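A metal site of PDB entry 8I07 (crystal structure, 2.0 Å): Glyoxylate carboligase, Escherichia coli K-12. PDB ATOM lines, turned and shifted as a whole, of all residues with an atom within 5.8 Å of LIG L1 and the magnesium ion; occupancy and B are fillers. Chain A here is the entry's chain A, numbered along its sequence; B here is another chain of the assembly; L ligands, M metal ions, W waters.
An oxygen (O2) of LIG L1 sits at hydrogen-bond distance from the backbone NH (N) of Asp 449 (2.9 Å). The backbone NH of Phe 448 is in hydrogen-bond range of an oxygen (O2) of LIG L1 (3.5 Å). The backbone NH of Ala 29 of chain B lies within hydrogen-bond range of an oxygen (O1) of LG2 L2, 2.9 Å away. The backbone carbonyl oxygen of Gly 420 lies within hydrogen-bond range of a nitrogen (N3) of LIG L1. An oxygen (O7) of LIG L1 lies within hydrogen-bond range of the backbone NH (N) of Gly 478 (3.3 Å). O7 of LIG L1 is in hydrogen-bond range of N of Leu 479, at 2.9 Å. The side-chain amide nitrogen (NE2) of Gln 116 of chain B sits close to a nitrogen (N3) of LIG L1 (3.2 Å). N of Asp 447 sits close to O3 of LIG L1 (3.2 Å). O7 of LIG L1 sits at hydrogen-bond distance from N of Leu 396 (2.8 Å). The backbone NH (N) of Ser 397 is in hydrogen-bond range of an oxygen (O6) of LIG L1, 3.0 Å away. A nitrogen (N2) of LIG L1 sits at hydrogen-bond distance from the backbone NH of Leu 422.
The side-chain carboxylate of Asp 447 lies close to the side-chain amide oxygen of Asn 473, at 3.3 Å. The backbone carbonyl oxygen (O) of Gly 420 lies within hydrogen-bond range of the side-chain amide nitrogen (NE2) of Gln 116 of chain B, at 3.3 Å. NE2 of Gln 116 of chain B sits at hydrogen-bond distance from O of Ala 419, 2.8 Å away. The side-chain carboxylate of Asp 447 sits close to the backbone NH of Ala 475 (3.2 Å). The backbone NH (N) of Gly 446 lies within hydrogen-bond range of the side-chain hydroxyl (OG) of Ser 397, at 3.3 Å. The side-chain carboxylate (OD2) of Asp 449 lies within hydrogen-bond range of the side-chain hydroxyl (OG) of Ser 445, 2.6 Å away.
Residues that only touch LIG L1: Asp 83 of chain B (3.3 Å), Pro 27 of chain B (3.4 Å), Gly 395 (3.5 Å), Gly 446 (3.5 Å), Leu 477 (3.5 Å), Ile 480 (3.6 Å), Thr 76 of chain B (3.6 Å), Pro 79 of chain B (3.6 Å), Ile 394 (3.6 Å), Val 52 of chain B (3.7 Å), Phe 452 (3.8 Å) and Val 26 of chain B (3.9 Å). Hydrophobic or aromatic side chains within 4 Å of LIG L1: Ile 394, Leu 396, Leu 422, Phe 448, Phe 452, Leu 477, Leu 479, Ile 480, Val 26 of chain B, Val 52 of chain B and Pro 79 of chain B. Of the 36 residues printed, 24 come within 4 Å of LIG L1.
Of the 36 residues printed, 3 come within 4 Å of the magnesium ion.
The magnesium ion is bound by OD1 of Asn 474, OD1 of Asp 447, O3 of LIG L1, O of Tyr 476, O5 of LIG L1 and water W4.
Water W4 lies within hydrogen-bond range of the backbone carbonyl oxygen (O) of Val 472 (2.7 Å), an oxygen (O6) of LIG L1 (2.9 Å), the side-chain amide nitrogen (ND2) of Asn 474 (3.3 Å) and the backbone NH (N) of Asp 447 (3.5 Å). Water W1 lies within hydrogen-bond range of an oxygen (O2) of LIG L1 (2.6 Å), the side-chain hydroxyl (OG) of Ser 397 (2.6 Å), the backbone NH (N) of Gly 446 (2.7 Å) and the backbone carbonyl oxygen (O) of Ile 394 (2.8 Å). Water W2 lies within hydrogen-bond range of O6 of LIG L1 (2.9 Å) and N of Ser 397 (3.5 Å). Water W3 lies within hydrogen-bond range of the backbone carbonyl oxygen (O) of Val 26 of chain B, the backbone NH (N) of Thr 76 of chain B and a nitrogen (N1) of LIG L1.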
ATOM      1  N   ILE A 394       8.441  -6.350 -18.850  1.00  0.00           N
ATOM      2  CA  ILE A 394       7.359  -5.427 -19.164  1.00  0.00           C
ATOM      3  C   ILE A 394       6.976  -4.665 -17.900  1.00  0.00           C
ATOM      4  O   ILE A 394       7.173  -5.140 -16.775  1.00  0.00           O
ATOM      5  CB  ILE A 394       6.138  -6.190 -19.756  1.00  0.00           C
ATOM      6  CG1 ILE A 394       5.068  -5.219 -20.287  1.00  0.00           C
ATOM      7  CG2 ILE A 394       5.516  -7.109 -18.721  1.00  0.00           C
ATOM      8  CD1 ILE A 394       4.049  -5.873 -21.201  1.00  0.00           C
ATOM      9  N   GLY A 395       6.399  -3.488 -18.083  1.00  0.00           N
ATOM     10  CA  GLY A 395       6.053  -2.589 -16.998  1.00  0.00           C
ATOM     11  C   GLY A 395       6.649  -1.206 -17.228  1.00  0.00           C
ATOM     12  O   GLY A 395       7.413  -0.978 -18.163  1.00  0.00           O
ATOM     13  N   LEU A 396       6.253  -0.265 -16.360  1.00  0.00           N
ATOM     14  CA  LEU A 396       6.908   1.043 -16.416  1.00  0.00           C
ATOM     15  C   LEU A 396       8.401   0.897 -16.153  1.00  0.00           C
ATOM     16  O   LEU A 396       9.224   1.624 -16.734  1.00  0.00           O
ATOM     17  CB  LEU A 396       6.257   2.016 -15.427  1.00  0.00           C
ATOM     18  CG  LEU A 396       4.801   2.388 -15.719  1.00  0.00           C
ATOM     19  CD1 LEU A 396       4.310   3.480 -14.740  1.00  0.00           C
ATOM     20  CD2 LEU A 396       4.629   2.840 -17.158  1.00  0.00           C
ATOM     21  N   SER A 397       8.761  -0.064 -15.317  1.00  0.00           N
ATOM     22  CA  SER A 397      10.150  -0.424 -15.096  1.00  0.00           C
ATOM     23  C   SER A 397      10.864  -0.641 -16.417  1.00  0.00           C
ATOM     24  O   SER A 397      11.902  -0.023 -16.683  1.00  0.00           O
ATOM     25  CB  SER A 397      10.192  -1.705 -14.262  1.00  0.00           C
ATOM     26  OG  SER A 397       9.336  -2.684 -14.895  1.00  0.00           O
ATOM     27  N   GLN A 398      10.306  -1.511 -17.272  1.00  0.00           N
ATOM     28  CA  GLN A 398      10.939  -1.887 -18.533  1.00  0.00           C
ATOM     29  C   GLN A 398      10.818  -0.790 -19.586  1.00  0.00           C
ATOM     30  O   GLN A 398      11.746  -0.583 -20.379  1.00  0.00           O
ATOM     31  CB  GLN A 398      10.344  -3.197 -19.069  1.00  0.00           C
ATOM     32  CG  GLN A 398      10.764  -3.577 -20.503  1.00  0.00           C
ATOM     33  CD  GLN A 398       9.705  -3.238 -21.567  1.00  0.00           C
ATOM     34  OE1 GLN A 398       8.653  -2.704 -21.256  1.00  0.00           O
ATOM     35  NE2 GLN A 398       9.992  -3.562 -22.845  1.00  0.00           N
ATOM     36  N   ALA A 419       5.485 -10.866 -26.404  1.00  0.00           N
ATOM     37  CA  ALA A 419       4.570 -11.509 -25.463  1.00  0.00           C
ATOM     38  C   ALA A 419       4.605 -10.920 -24.057  1.00  0.00           C
ATOM     39  O   ALA A 419       3.570 -10.909 -23.374  1.00  0.00           O
ATOM     40  CB  ALA A 419       4.866 -13.017 -25.396  1.00  0.00           C
ATOM     41  N   GLY A 420       5.765 -10.492 -23.568  1.00  0.00           N
ATOM     42  CA  GLY A 420       5.831  -9.823 -22.283  1.00  0.00           C
ATOM     43  C   GLY A 420       5.211 -10.538 -21.073  1.00  0.00           C
ATOM     44  O   GLY A 420       4.543  -9.908 -20.258  1.00  0.00           O
ATOM     45  N   PRO A 421       5.420 -11.848 -20.918  1.00  0.00           N
ATOM     46  CA  PRO A 421       4.858 -12.546 -19.737  1.00  0.00           C
ATOM     47  C   PRO A 421       5.534 -12.124 -18.441  1.00  0.00           C
ATOM     48  O   PRO A 421       6.755 -12.221 -18.298  1.00  0.00           O
ATOM     49  CB  PRO A 421       5.130 -14.016 -20.040  1.00  0.00           C
ATOM     50  CG  PRO A 421       6.328 -13.994 -20.938  1.00  0.00           C
ATOM     51  CD  PRO A 421       6.190 -12.749 -21.786  1.00  0.00           C
ATOM     52  N   LEU A 422       4.722 -11.710 -17.462  1.00  0.00           N
ATOM     53  CA  LEU A 422       5.277 -11.374 -16.163  1.00  0.00           C
ATOM     54  C   LEU A 422       5.910 -12.601 -15.528  1.00  0.00           C
ATOM     55  O   LEU A 422       5.475 -13.725 -15.730  1.00  0.00           O
ATOM     56  CB  LEU A 422       4.192 -10.786 -15.242  1.00  0.00           C
ATOM     57  CG  LEU A 422       3.758  -9.357 -15.577  1.00  0.00           C
ATOM     58  CD1 LEU A 422       2.395  -9.070 -14.944  1.00  0.00           C
ATOM     59  CD2 LEU A 422       4.817  -8.284 -15.150  1.00  0.00           C
ATOM     60  N   SER A 445      13.387  -5.292 -13.056  1.00  0.00           N
ATOM     61  CA  SER A 445      11.995  -5.685 -12.826  1.00  0.00           C
ATOM     62  C   SER A 445      11.301  -4.614 -12.011  1.00  0.00           C
ATOM     63  O   SER A 445      11.914  -3.978 -11.148  1.00  0.00           O
ATOM     64  CB  SER A 445      11.858  -6.992 -12.014  1.00  0.00           C
ATOM     65  OG  SER A 445      12.156  -8.156 -12.757  1.00  0.00           O
ATOM     66  N   GLY A 446       9.978  -4.469 -12.236  1.00  0.00           N
ATOM     67  CA  GLY A 446       9.105  -3.913 -11.220  1.00  0.00           C
ATOM     68  C   GLY A 446       8.728  -4.960 -10.171  1.00  0.00           C
ATOM     69  O   GLY A 446       9.035  -6.146 -10.323  1.00  0.00           O
ATOM     70  N   ASP A 447       8.052  -4.512  -9.099  1.00  0.00           N
ATOM     71  CA  ASP A 447       7.752  -5.430  -8.005  1.00  0.00           C
ATOM     72  C   ASP A 447       6.841  -6.576  -8.446  1.00  0.00           C
ATOM     73  O   ASP A 447       7.033  -7.728  -8.022  1.00  0.00           O
ATOM     74  CB  ASP A 447       7.166  -4.703  -6.781  1.00  0.00           C
ATOM     75  CG  ASP A 447       6.128  -3.629  -7.132  1.00  0.00           C
ATOM     76  OD1 ASP A 447       6.304  -2.836  -8.082  1.00  0.00           O
ATOM     77  OD2 ASP A 447       5.140  -3.537  -6.378  1.00  0.00           O
ATOM     78  N   PHE A 448       5.859  -6.299  -9.300  1.00  0.00           N
ATOM     79  CA  PHE A 448       4.878  -7.340  -9.653  1.00  0.00           C
ATOM     80  C   PHE A 448       5.532  -8.426 -10.500  1.00  0.00           C
ATOM     81  O   PHE A 448       5.400  -9.614 -10.214  1.00  0.00           O
ATOM     82  CB  PHE A 448       3.701  -6.697 -10.383  1.00  0.00           C
ATOM     83  CG  PHE A 448       2.418  -7.535 -10.395  1.00  0.00           C
ATOM     84  CD1 PHE A 448       1.909  -8.061  -9.221  1.00  0.00           C
ATOM     85  CD2 PHE A 448       1.716  -7.708 -11.561  1.00  0.00           C
ATOM     86  CE1 PHE A 448       0.708  -8.801  -9.220  1.00  0.00           C
ATOM     87  CE2 PHE A 448       0.521  -8.435 -11.584  1.00  0.00           C
ATOM     88  CZ  PHE A 448       0.010  -8.976 -10.396  1.00  0.00           C
ATOM     89  N   ASP A 449       6.308  -8.024 -11.522  1.00  0.00           N
ATOM     90  CA  ASP A 449       7.066  -8.975 -12.314  1.00  0.00           C
ATOM     91  C   ASP A 449       8.005  -9.799 -11.443  1.00  0.00           C
ATOM     92  O   ASP A 449       8.108 -11.020 -11.602  1.00  0.00           O
ATOM     93  CB  ASP A 449       7.848  -8.201 -13.395  1.00  0.00           C
ATOM     94  CG  ASP A 449       8.976  -9.000 -14.033  1.00  0.00           C
ATOM     95  OD1 ASP A 449       8.806 -10.173 -14.412  1.00  0.00           O
ATOM     96  OD2 ASP A 449      10.054  -8.409 -14.233  1.00  0.00           O
ATOM     97  N   PHE A 450       8.672  -9.149 -10.488  1.00  0.00           N
ATOM     98  CA  PHE A 450       9.610  -9.832  -9.602  1.00  0.00           C
ATOM     99  C   PHE A 450       8.906 -10.906  -8.761  1.00  0.00           C
ATOM    100  O   PHE A 450       9.492 -11.955  -8.479  1.00  0.00           O
ATOM    101  CB  PHE A 450      10.288  -8.795  -8.697  1.00  0.00           C
ATOM    102  CG  PHE A 450      11.497  -9.303  -7.950  1.00  0.00           C
ATOM    103  CD1 PHE A 450      12.672  -9.566  -8.612  1.00  0.00           C
ATOM    104  CD2 PHE A 450      11.447  -9.451  -6.577  1.00  0.00           C
ATOM    105  CE1 PHE A 450      13.779 -10.017  -7.917  1.00  0.00           C
ATOM    106  CE2 PHE A 450      12.562  -9.891  -5.882  1.00  0.00           C
ATOM    107  CZ  PHE A 450      13.721 -10.177  -6.543  1.00  0.00           C
ATOM    108  N   PHE A 452       6.079 -12.763  -9.530  1.00  0.00           N
ATOM    109  CA  PHE A 452       5.452 -13.896 -10.225  1.00  0.00           C
ATOM    110  C   PHE A 452       6.242 -15.194 -10.031  1.00  0.00           C
ATOM    111  O   PHE A 452       5.678 -16.229  -9.645  1.00  0.00           O
ATOM    112  CB  PHE A 452       5.329 -13.605 -11.722  1.00  0.00           C
ATOM    113  CG  PHE A 452       3.966 -13.135 -12.173  1.00  0.00           C
ATOM    114  CD1 PHE A 452       3.414 -11.964 -11.654  1.00  0.00           C
ATOM    115  CD2 PHE A 452       3.269 -13.817 -13.151  1.00  0.00           C
ATOM    116  CE1 PHE A 452       2.168 -11.520 -12.089  1.00  0.00           C
ATOM    117  CE2 PHE A 452       2.036 -13.383 -13.590  1.00  0.00           C
ATOM    118  CZ  PHE A 452       1.483 -12.228 -13.056  1.00  0.00           C
ATOM    119  N   VAL A 472      12.696  -2.152  -9.023  1.00  0.00           N
ATOM    120  CA  VAL A 472      12.171  -0.804  -8.785  1.00  0.00           C
ATOM    121  C   VAL A 472      10.746  -0.965  -8.280  1.00  0.00           C
ATOM    122  O   VAL A 472       9.854  -1.393  -9.026  1.00  0.00           O
ATOM    123  CB  VAL A 472      12.267   0.086 -10.032  1.00  0.00           C
ATOM    124  CG1 VAL A 472      13.733   0.246 -10.457  1.00  0.00           C
ATOM    125  CG2 VAL A 472      11.433  -0.445 -11.222  1.00  0.00           C
ATOM    126  N   ASN A 473      10.530  -0.624  -7.004  1.00  0.00           N
ATOM    127  CA  ASN A 473       9.338  -1.032  -6.259  1.00  0.00           C
ATOM    128  C   ASN A 473       8.434   0.174  -6.040  1.00  0.00           C
ATOM    129  O   ASN A 473       8.779   1.075  -5.281  1.00  0.00           O
ATOM    130  CB  ASN A 473       9.746  -1.659  -4.918  1.00  0.00           C
ATOM    131  CG  ASN A 473       8.561  -2.114  -4.092  1.00  0.00           C
ATOM    132  OD1 ASN A 473       7.425  -2.076  -4.550  1.00  0.00           O
ATOM    133  ND2 ASN A 473       8.820  -2.564  -2.875  1.00  0.00           N
ATOM    134  N   ASN A 474       7.268   0.177  -6.696  1.00  0.00           N
ATOM    135  CA  ASN A 474       6.276   1.211  -6.460  1.00  0.00           C
ATOM    136  C   ASN A 474       5.012   0.679  -5.782  1.00  0.00           C
ATOM    137  O   ASN A 474       4.008   1.385  -5.711  1.00  0.00           O
ATOM    138  CB  ASN A 474       5.930   1.925  -7.781  1.00  0.00           C
ATOM    139  CG  ASN A 474       5.480   0.970  -8.903  1.00  0.00           C
ATOM    140  OD1 ASN A 474       5.095  -0.173  -8.653  1.00  0.00           O
ATOM    141  ND2 ASN A 474       5.541   1.447 -10.145  1.00  0.00           N
ATOM    142  N   ALA A 475       5.030  -0.554  -5.288  1.00  0.00           N
ATOM    143  CA  ALA A 475       3.836  -1.201  -4.730  1.00  0.00           C
ATOM    144  C   ALA A 475       2.627  -1.022  -5.648  1.00  0.00           C
ATOM    145  O   ALA A 475       1.497  -0.840  -5.189  1.00  0.00           O
ATOM    146  CB  ALA A 475       3.546  -0.698  -3.316  1.00  0.00           C
ATOM    147  N   TYR A 476       2.857  -1.128  -6.952  1.00  0.00           N
ATOM    148  CA  TYR A 476       1.810  -0.894  -7.949  1.00  0.00           C
ATOM    149  C   TYR A 476       2.053  -1.807  -9.143  1.00  0.00           C
ATOM    150  O   TYR A 476       3.193  -2.142  -9.457  1.00  0.00           O
ATOM    151  CB  TYR A 476       1.830   0.567  -8.439  1.00  0.00           C
ATOM    152  CG  TYR A 476       0.735   1.531  -7.989  1.00  0.00           C
ATOM    153  CD1 TYR A 476      -0.538   1.467  -8.522  1.00  0.00           C
ATOM    154  CD2 TYR A 476       1.015   2.554  -7.090  1.00  0.00           C
ATOM    155  CE1 TYR A 476      -1.517   2.371  -8.135  1.00  0.00           C
ATOM    156  CE2 TYR A 476       0.060   3.466  -6.718  1.00  0.00           C
ATOM    157  CZ  TYR A 476      -1.213   3.367  -7.230  1.00  0.00           C
ATOM    158  OH  TYR A 476      -2.180   4.280  -6.852  1.00  0.00           O
ATOM    159  N   LEU A 477       0.967  -2.187  -9.840  1.00  0.00           N
ATOM    160  CA  LEU A 477       1.089  -2.541 -11.256  1.00  0.00           C
ATOM    161  C   LEU A 477       1.065  -1.211 -12.009  1.00  0.00           C
ATOM    162  O   LEU A 477       0.017  -0.710 -12.434  1.00  0.00           O
ATOM    163  CB  LEU A 477      -0.023  -3.479 -11.739  1.00  0.00           C
ATOM    164  CG  LEU A 477      -0.779  -4.495 -10.866  1.00  0.00           C
ATOM    165  CD1 LEU A 477      -1.578  -5.521 -11.697  1.00  0.00           C
ATOM    166  CD2 LEU A 477       0.062  -5.156  -9.779  1.00  0.00           C
ATOM    167  N   GLY A 478       2.230  -0.577 -12.103  1.00  0.00           N
ATOM    168  CA  GLY A 478       2.262   0.824 -12.484  1.00  0.00           C
ATOM    169  C   GLY A 478       1.808   1.070 -13.910  1.00  0.00           C
ATOM    170  O   GLY A 478       1.070   2.021 -14.186  1.00  0.00           O
ATOM    171  N   LEU A 479       2.188   0.184 -14.833  1.00  0.00           N
ATOM    172  CA  LEU A 479       1.742   0.364 -16.205  1.00  0.00           C
ATOM    173  C   LEU A 479       0.215   0.267 -16.292  1.00  0.00           C
ATOM    174  O   LEU A 479      -0.414   1.015 -17.043  1.00  0.00           O
ATOM    175  CB  LEU A 479       2.408  -0.670 -17.128  1.00  0.00           C
ATOM    176  CG  LEU A 479       2.024  -0.626 -18.616  1.00  0.00           C
ATOM    177  CD1 LEU A 479       2.266   0.748 -19.221  1.00  0.00           C
ATOM    178  CD2 LEU A 479       2.773  -1.702 -19.398  1.00  0.00           C
ATOM    179  N   ILE A 480      -0.388  -0.609 -15.493  1.00  0.00           N
ATOM    180  CA  ILE A 480      -1.837  -0.764 -15.590  1.00  0.00           C
ATOM    181  C   ILE A 480      -2.526   0.414 -14.936  1.00  0.00           C
ATOM    182  O   ILE A 480      -3.537   0.903 -15.443  1.00  0.00           O
ATOM    183  CB  ILE A 480      -2.295  -2.120 -14.989  1.00  0.00           C
ATOM    184  CG1 ILE A 480      -1.429  -3.260 -15.548  1.00  0.00           C
ATOM    185  CG2 ILE A 480      -3.771  -2.374 -15.321  1.00  0.00           C
ATOM    186  CD1 ILE A 480      -1.269  -3.231 -17.068  1.00  0.00           C
ATOM    187  N   LEU A 495      -0.517  -2.947  -4.633  1.00  0.00           N
ATOM    188  CA  LEU A 495       0.065  -4.092  -3.952  1.00  0.00           C
ATOM    189  C   LEU A 495       0.457  -3.783  -2.517  1.00  0.00           C
ATOM    190  O   LEU A 495       0.963  -4.679  -1.823  1.00  0.00           O
ATOM    191  CB  LEU A 495       1.290  -4.587  -4.729  1.00  0.00           C
ATOM    192  CG  LEU A 495       1.021  -5.127  -6.133  1.00  0.00           C
ATOM    193  CD1 LEU A 495       2.310  -5.318  -6.906  1.00  0.00           C
ATOM    194  CD2 LEU A 495       0.202  -6.455  -6.085  1.00  0.00           C
ATOM    195  N   VAL B  26      -5.871 -10.577 -12.507  1.00  0.00           N
ATOM    196  CA  VAL B  26      -4.746  -9.670 -12.724  1.00  0.00           C
ATOM    197  C   VAL B  26      -5.141  -8.751 -13.878  1.00  0.00           C
ATOM    198  O   VAL B  26      -5.289  -9.234 -15.014  1.00  0.00           O
ATOM    199  CB  VAL B  26      -3.453 -10.436 -13.049  1.00  0.00           C
ATOM    200  CG1 VAL B  26      -2.305  -9.444 -13.402  1.00  0.00           C
ATOM    201  CG2 VAL B  26      -3.058 -11.355 -11.894  1.00  0.00           C
ATOM    202  N   PRO B  27      -5.380  -7.464 -13.632  1.00  0.00           N
ATOM    203  CA  PRO B  27      -5.796  -6.572 -14.732  1.00  0.00           C
ATOM    204  C   PRO B  27      -4.646  -6.304 -15.705  1.00  0.00           C
ATOM    205  O   PRO B  27      -3.479  -6.587 -15.431  1.00  0.00           O
ATOM    206  CB  PRO B  27      -6.220  -5.288 -14.002  1.00  0.00           C
ATOM    207  CG  PRO B  27      -5.359  -5.267 -12.770  1.00  0.00           C
ATOM    208  CD  PRO B  27      -5.207  -6.725 -12.362  1.00  0.00           C
ATOM    209  N   GLY B  28      -5.024  -5.837 -16.892  1.00  0.00           N
ATOM    210  CA  GLY B  28      -4.076  -5.368 -17.894  1.00  0.00           C
ATOM    211  C   GLY B  28      -4.828  -4.489 -18.857  1.00  0.00           C
ATOM    212  O   GLY B  28      -6.053  -4.367 -18.788  1.00  0.00           O
ATOM    213  N   ALA B  29      -4.092  -3.899 -19.803  1.00  0.00           N
ATOM    214  CA  ALA B  29      -4.692  -2.893 -20.683  1.00  0.00           C
ATOM    215  C   ALA B  29      -5.878  -3.449 -21.463  1.00  0.00           C
ATOM    216  O   ALA B  29      -6.906  -2.773 -21.611  1.00  0.00           O
ATOM    217  CB  ALA B  29      -3.618  -2.341 -21.630  1.00  0.00           C
ATOM    218  N   VAL B  52      -0.877 -14.951 -12.593  1.00  0.00           N
ATOM    219  CA  VAL B  52      -2.147 -15.301 -13.231  1.00  0.00           C
ATOM    220  C   VAL B  52      -2.477 -16.757 -12.952  1.00  0.00           C
ATOM    221  O   VAL B  52      -3.643 -17.107 -12.762  1.00  0.00           O
ATOM    222  CB  VAL B  52      -2.118 -15.009 -14.740  1.00  0.00           C
ATOM    223  CG1 VAL B  52      -3.275 -15.697 -15.452  1.00  0.00           C
ATOM    224  CG2 VAL B  52      -2.190 -13.493 -14.993  1.00  0.00           C
ATOM    225  N   THR B  76      -5.643 -10.377 -18.683  1.00  0.00           N
ATOM    226  CA  THR B  76      -5.495  -9.560 -19.879  1.00  0.00           C
ATOM    227  C   THR B  76      -5.235 -10.476 -21.089  1.00  0.00           C
ATOM    228  O   THR B  76      -5.461 -11.697 -21.036  1.00  0.00           O
ATOM    229  CB  THR B  76      -4.404  -8.506 -19.655  1.00  0.00           C
ATOM    230  OG1 THR B  76      -4.543  -7.455 -20.614  1.00  0.00           O
ATOM    231  CG2 THR B  76      -3.003  -9.118 -19.766  1.00  0.00           C
ATOM    232  N   PRO B  79      -0.099 -13.386 -22.720  1.00  0.00           N
ATOM    233  CA  PRO B  79       0.402 -14.386 -21.758  1.00  0.00           C
ATOM    234  C   PRO B  79      -0.549 -14.666 -20.590  1.00  0.00           C
ATOM    235  O   PRO B  79      -0.377 -15.684 -19.904  1.00  0.00           O
ATOM    236  CB  PRO B  79       1.732 -13.794 -21.275  1.00  0.00           C
ATOM    237  CG  PRO B  79       1.504 -12.311 -21.377  1.00  0.00           C
ATOM    238  CD  PRO B  79       0.699 -12.146 -22.674  1.00  0.00           C
ATOM    239  N   ALA B  80      -1.499 -13.785 -20.285  1.00  0.00           N
ATOM    240  CA  ALA B  80      -2.462 -14.092 -19.235  1.00  0.00           C
ATOM    241  C   ALA B  80      -3.276 -15.334 -19.582  1.00  0.00           C
ATOM    242  O   ALA B  80      -3.395 -16.251 -18.775  1.00  0.00           O
ATOM    243  CB  ALA B  80      -3.394 -12.891 -18.991  1.00  0.00           C
ATOM    244  N   ASP B  83      -1.207 -18.425 -19.288  1.00  0.00           N
ATOM    245  CA  ASP B  83      -1.017 -18.767 -17.873  1.00  0.00           C
ATOM    246  C   ASP B  83      -2.254 -19.417 -17.242  1.00  0.00           C
ATOM    247  O   ASP B  83      -2.177 -19.794 -16.066  1.00  0.00           O
ATOM    248  CB  ASP B  83      -0.664 -17.519 -17.055  1.00  0.00           C
ATOM    249  CG  ASP B  83       0.798 -17.122 -17.163  1.00  0.00           C
ATOM    250  OD1 ASP B  83       1.631 -17.852 -17.750  1.00  0.00           O
ATOM    251  OD2 ASP B  83       1.106 -16.031 -16.657  1.00  0.00           O
ATOM    252  N   GLN B 116       1.027  -8.597 -27.645  1.00  0.00           N
ATOM    253  CA  GLN B 116       0.375  -9.487 -26.673  1.00  0.00           C
ATOM    254  C   GLN B 116      -0.982 -10.007 -27.152  1.00  0.00           C
ATOM    255  O   GLN B 116      -1.956 -10.022 -26.406  1.00  0.00           O
ATOM    256  CB  GLN B 116       0.219  -8.776 -25.314  1.00  0.00           C
ATOM    257  CG  GLN B 116       1.533  -8.562 -24.590  1.00  0.00           C
ATOM    258  CD  GLN B 116       1.349  -8.205 -23.109  1.00  0.00           C
ATOM    259  OE1 GLN B 116       0.538  -7.338 -22.761  1.00  0.00           O
ATOM    260  NE2 GLN B 116       2.123  -8.856 -22.234  1.00  0.00           N
HETATM  261  N1  LIG L   1      -0.462 -10.857 -16.874  1.00  0.00           N
HETATM  262  C1  LIG L   1       0.655 -11.374 -17.419  1.00  0.00           C
HETATM  263  C2  LIG L   1       0.908 -12.830 -17.207  1.00  0.00           C
HETATM  264  N2  LIG L   1       1.570 -10.700 -18.128  1.00  0.00           N
HETATM  265  C3  LIG L   1       1.344  -9.387 -18.335  1.00  0.00           C
HETATM  266  N3  LIG L   1       2.267  -8.727 -19.059  1.00  0.00           N
HETATM  267  C4  LIG L   1       0.200  -8.727 -17.762  1.00  0.00           C
HETATM  268  C5  LIG L   1      -0.659  -9.548 -17.069  1.00  0.00           C
HETATM  269  C6  LIG L   1      -0.124  -7.253 -17.961  1.00  0.00           C
HETATM  270  N4  LIG L   1       0.854  -6.320 -17.348  1.00  0.00           N
HETATM  271  C7  LIG L   1       1.777  -5.660 -18.040  1.00  0.00           C
HETATM  272  S1  LIG L   1       2.716  -4.638 -17.071  1.00  0.00           S
HETATM  273  C8  LIG L   1       1.802  -5.072 -15.671  1.00  0.00           C
HETATM  274  C9  LIG L   1       0.839  -5.993 -15.986  1.00  0.00           C
HETATM  275  C10 LIG L   1      -0.139  -6.626 -15.058  1.00  0.00           C
HETATM  276  C11 LIG L   1       2.167  -4.490 -14.333  1.00  0.00           C
HETATM  277  C12 LIG L   1       3.661  -4.445 -14.133  1.00  0.00           C
HETATM  278  O1  LIG L   1       3.954  -4.169 -12.735  1.00  0.00           O
HETATM  279  P1  LIG L   1       5.407  -4.114 -12.158  1.00  0.00           P
HETATM  280  O2  LIG L   1       6.191  -5.341 -12.633  1.00  0.00           O
HETATM  281  O3  LIG L   1       5.343  -3.759 -10.722  1.00  0.00           O
HETATM  282  O4  LIG L   1       5.928  -2.825 -12.926  1.00  0.00           O
HETATM  283  P2  LIG L   1       5.639  -1.268 -12.906  1.00  0.00           P
HETATM  284  O5  LIG L   1       4.890  -0.948 -11.648  1.00  0.00           O
HETATM  285  O6  LIG L   1       6.986  -0.619 -13.015  1.00  0.00           O
HETATM  286  O7  LIG L   1       4.755  -1.035 -14.129  1.00  0.00           O
HETATM  287  C1  LG2 L   2      -0.556  -3.615 -20.373  1.00  0.00           C
HETATM  288  C2  LG2 L   2      -0.379  -2.857 -21.697  1.00  0.00           C
HETATM  289  O1  LG2 L   2      -1.321  -4.526 -20.291  1.00  0.00           O
HETATM  290  O2  LG2 L   2       0.818  -3.232 -22.319  1.00  0.00           O
HETATM  291 MG    MG M   1       5.336  -1.916  -9.704  1.00  0.00          MG
HETATM  292  O   HOH W   1       8.176  -4.944 -14.213  1.00  0.00           O
HETATM  293  O   HOH W   2       8.492   1.831 -12.388  1.00  0.00           O
HETATM  294  O   HOH W   3      -3.609 -10.555 -16.616  1.00  0.00           O
HETATM  295  O   HOH W   4       7.443  -1.274 -10.255  1.00  0.00           O
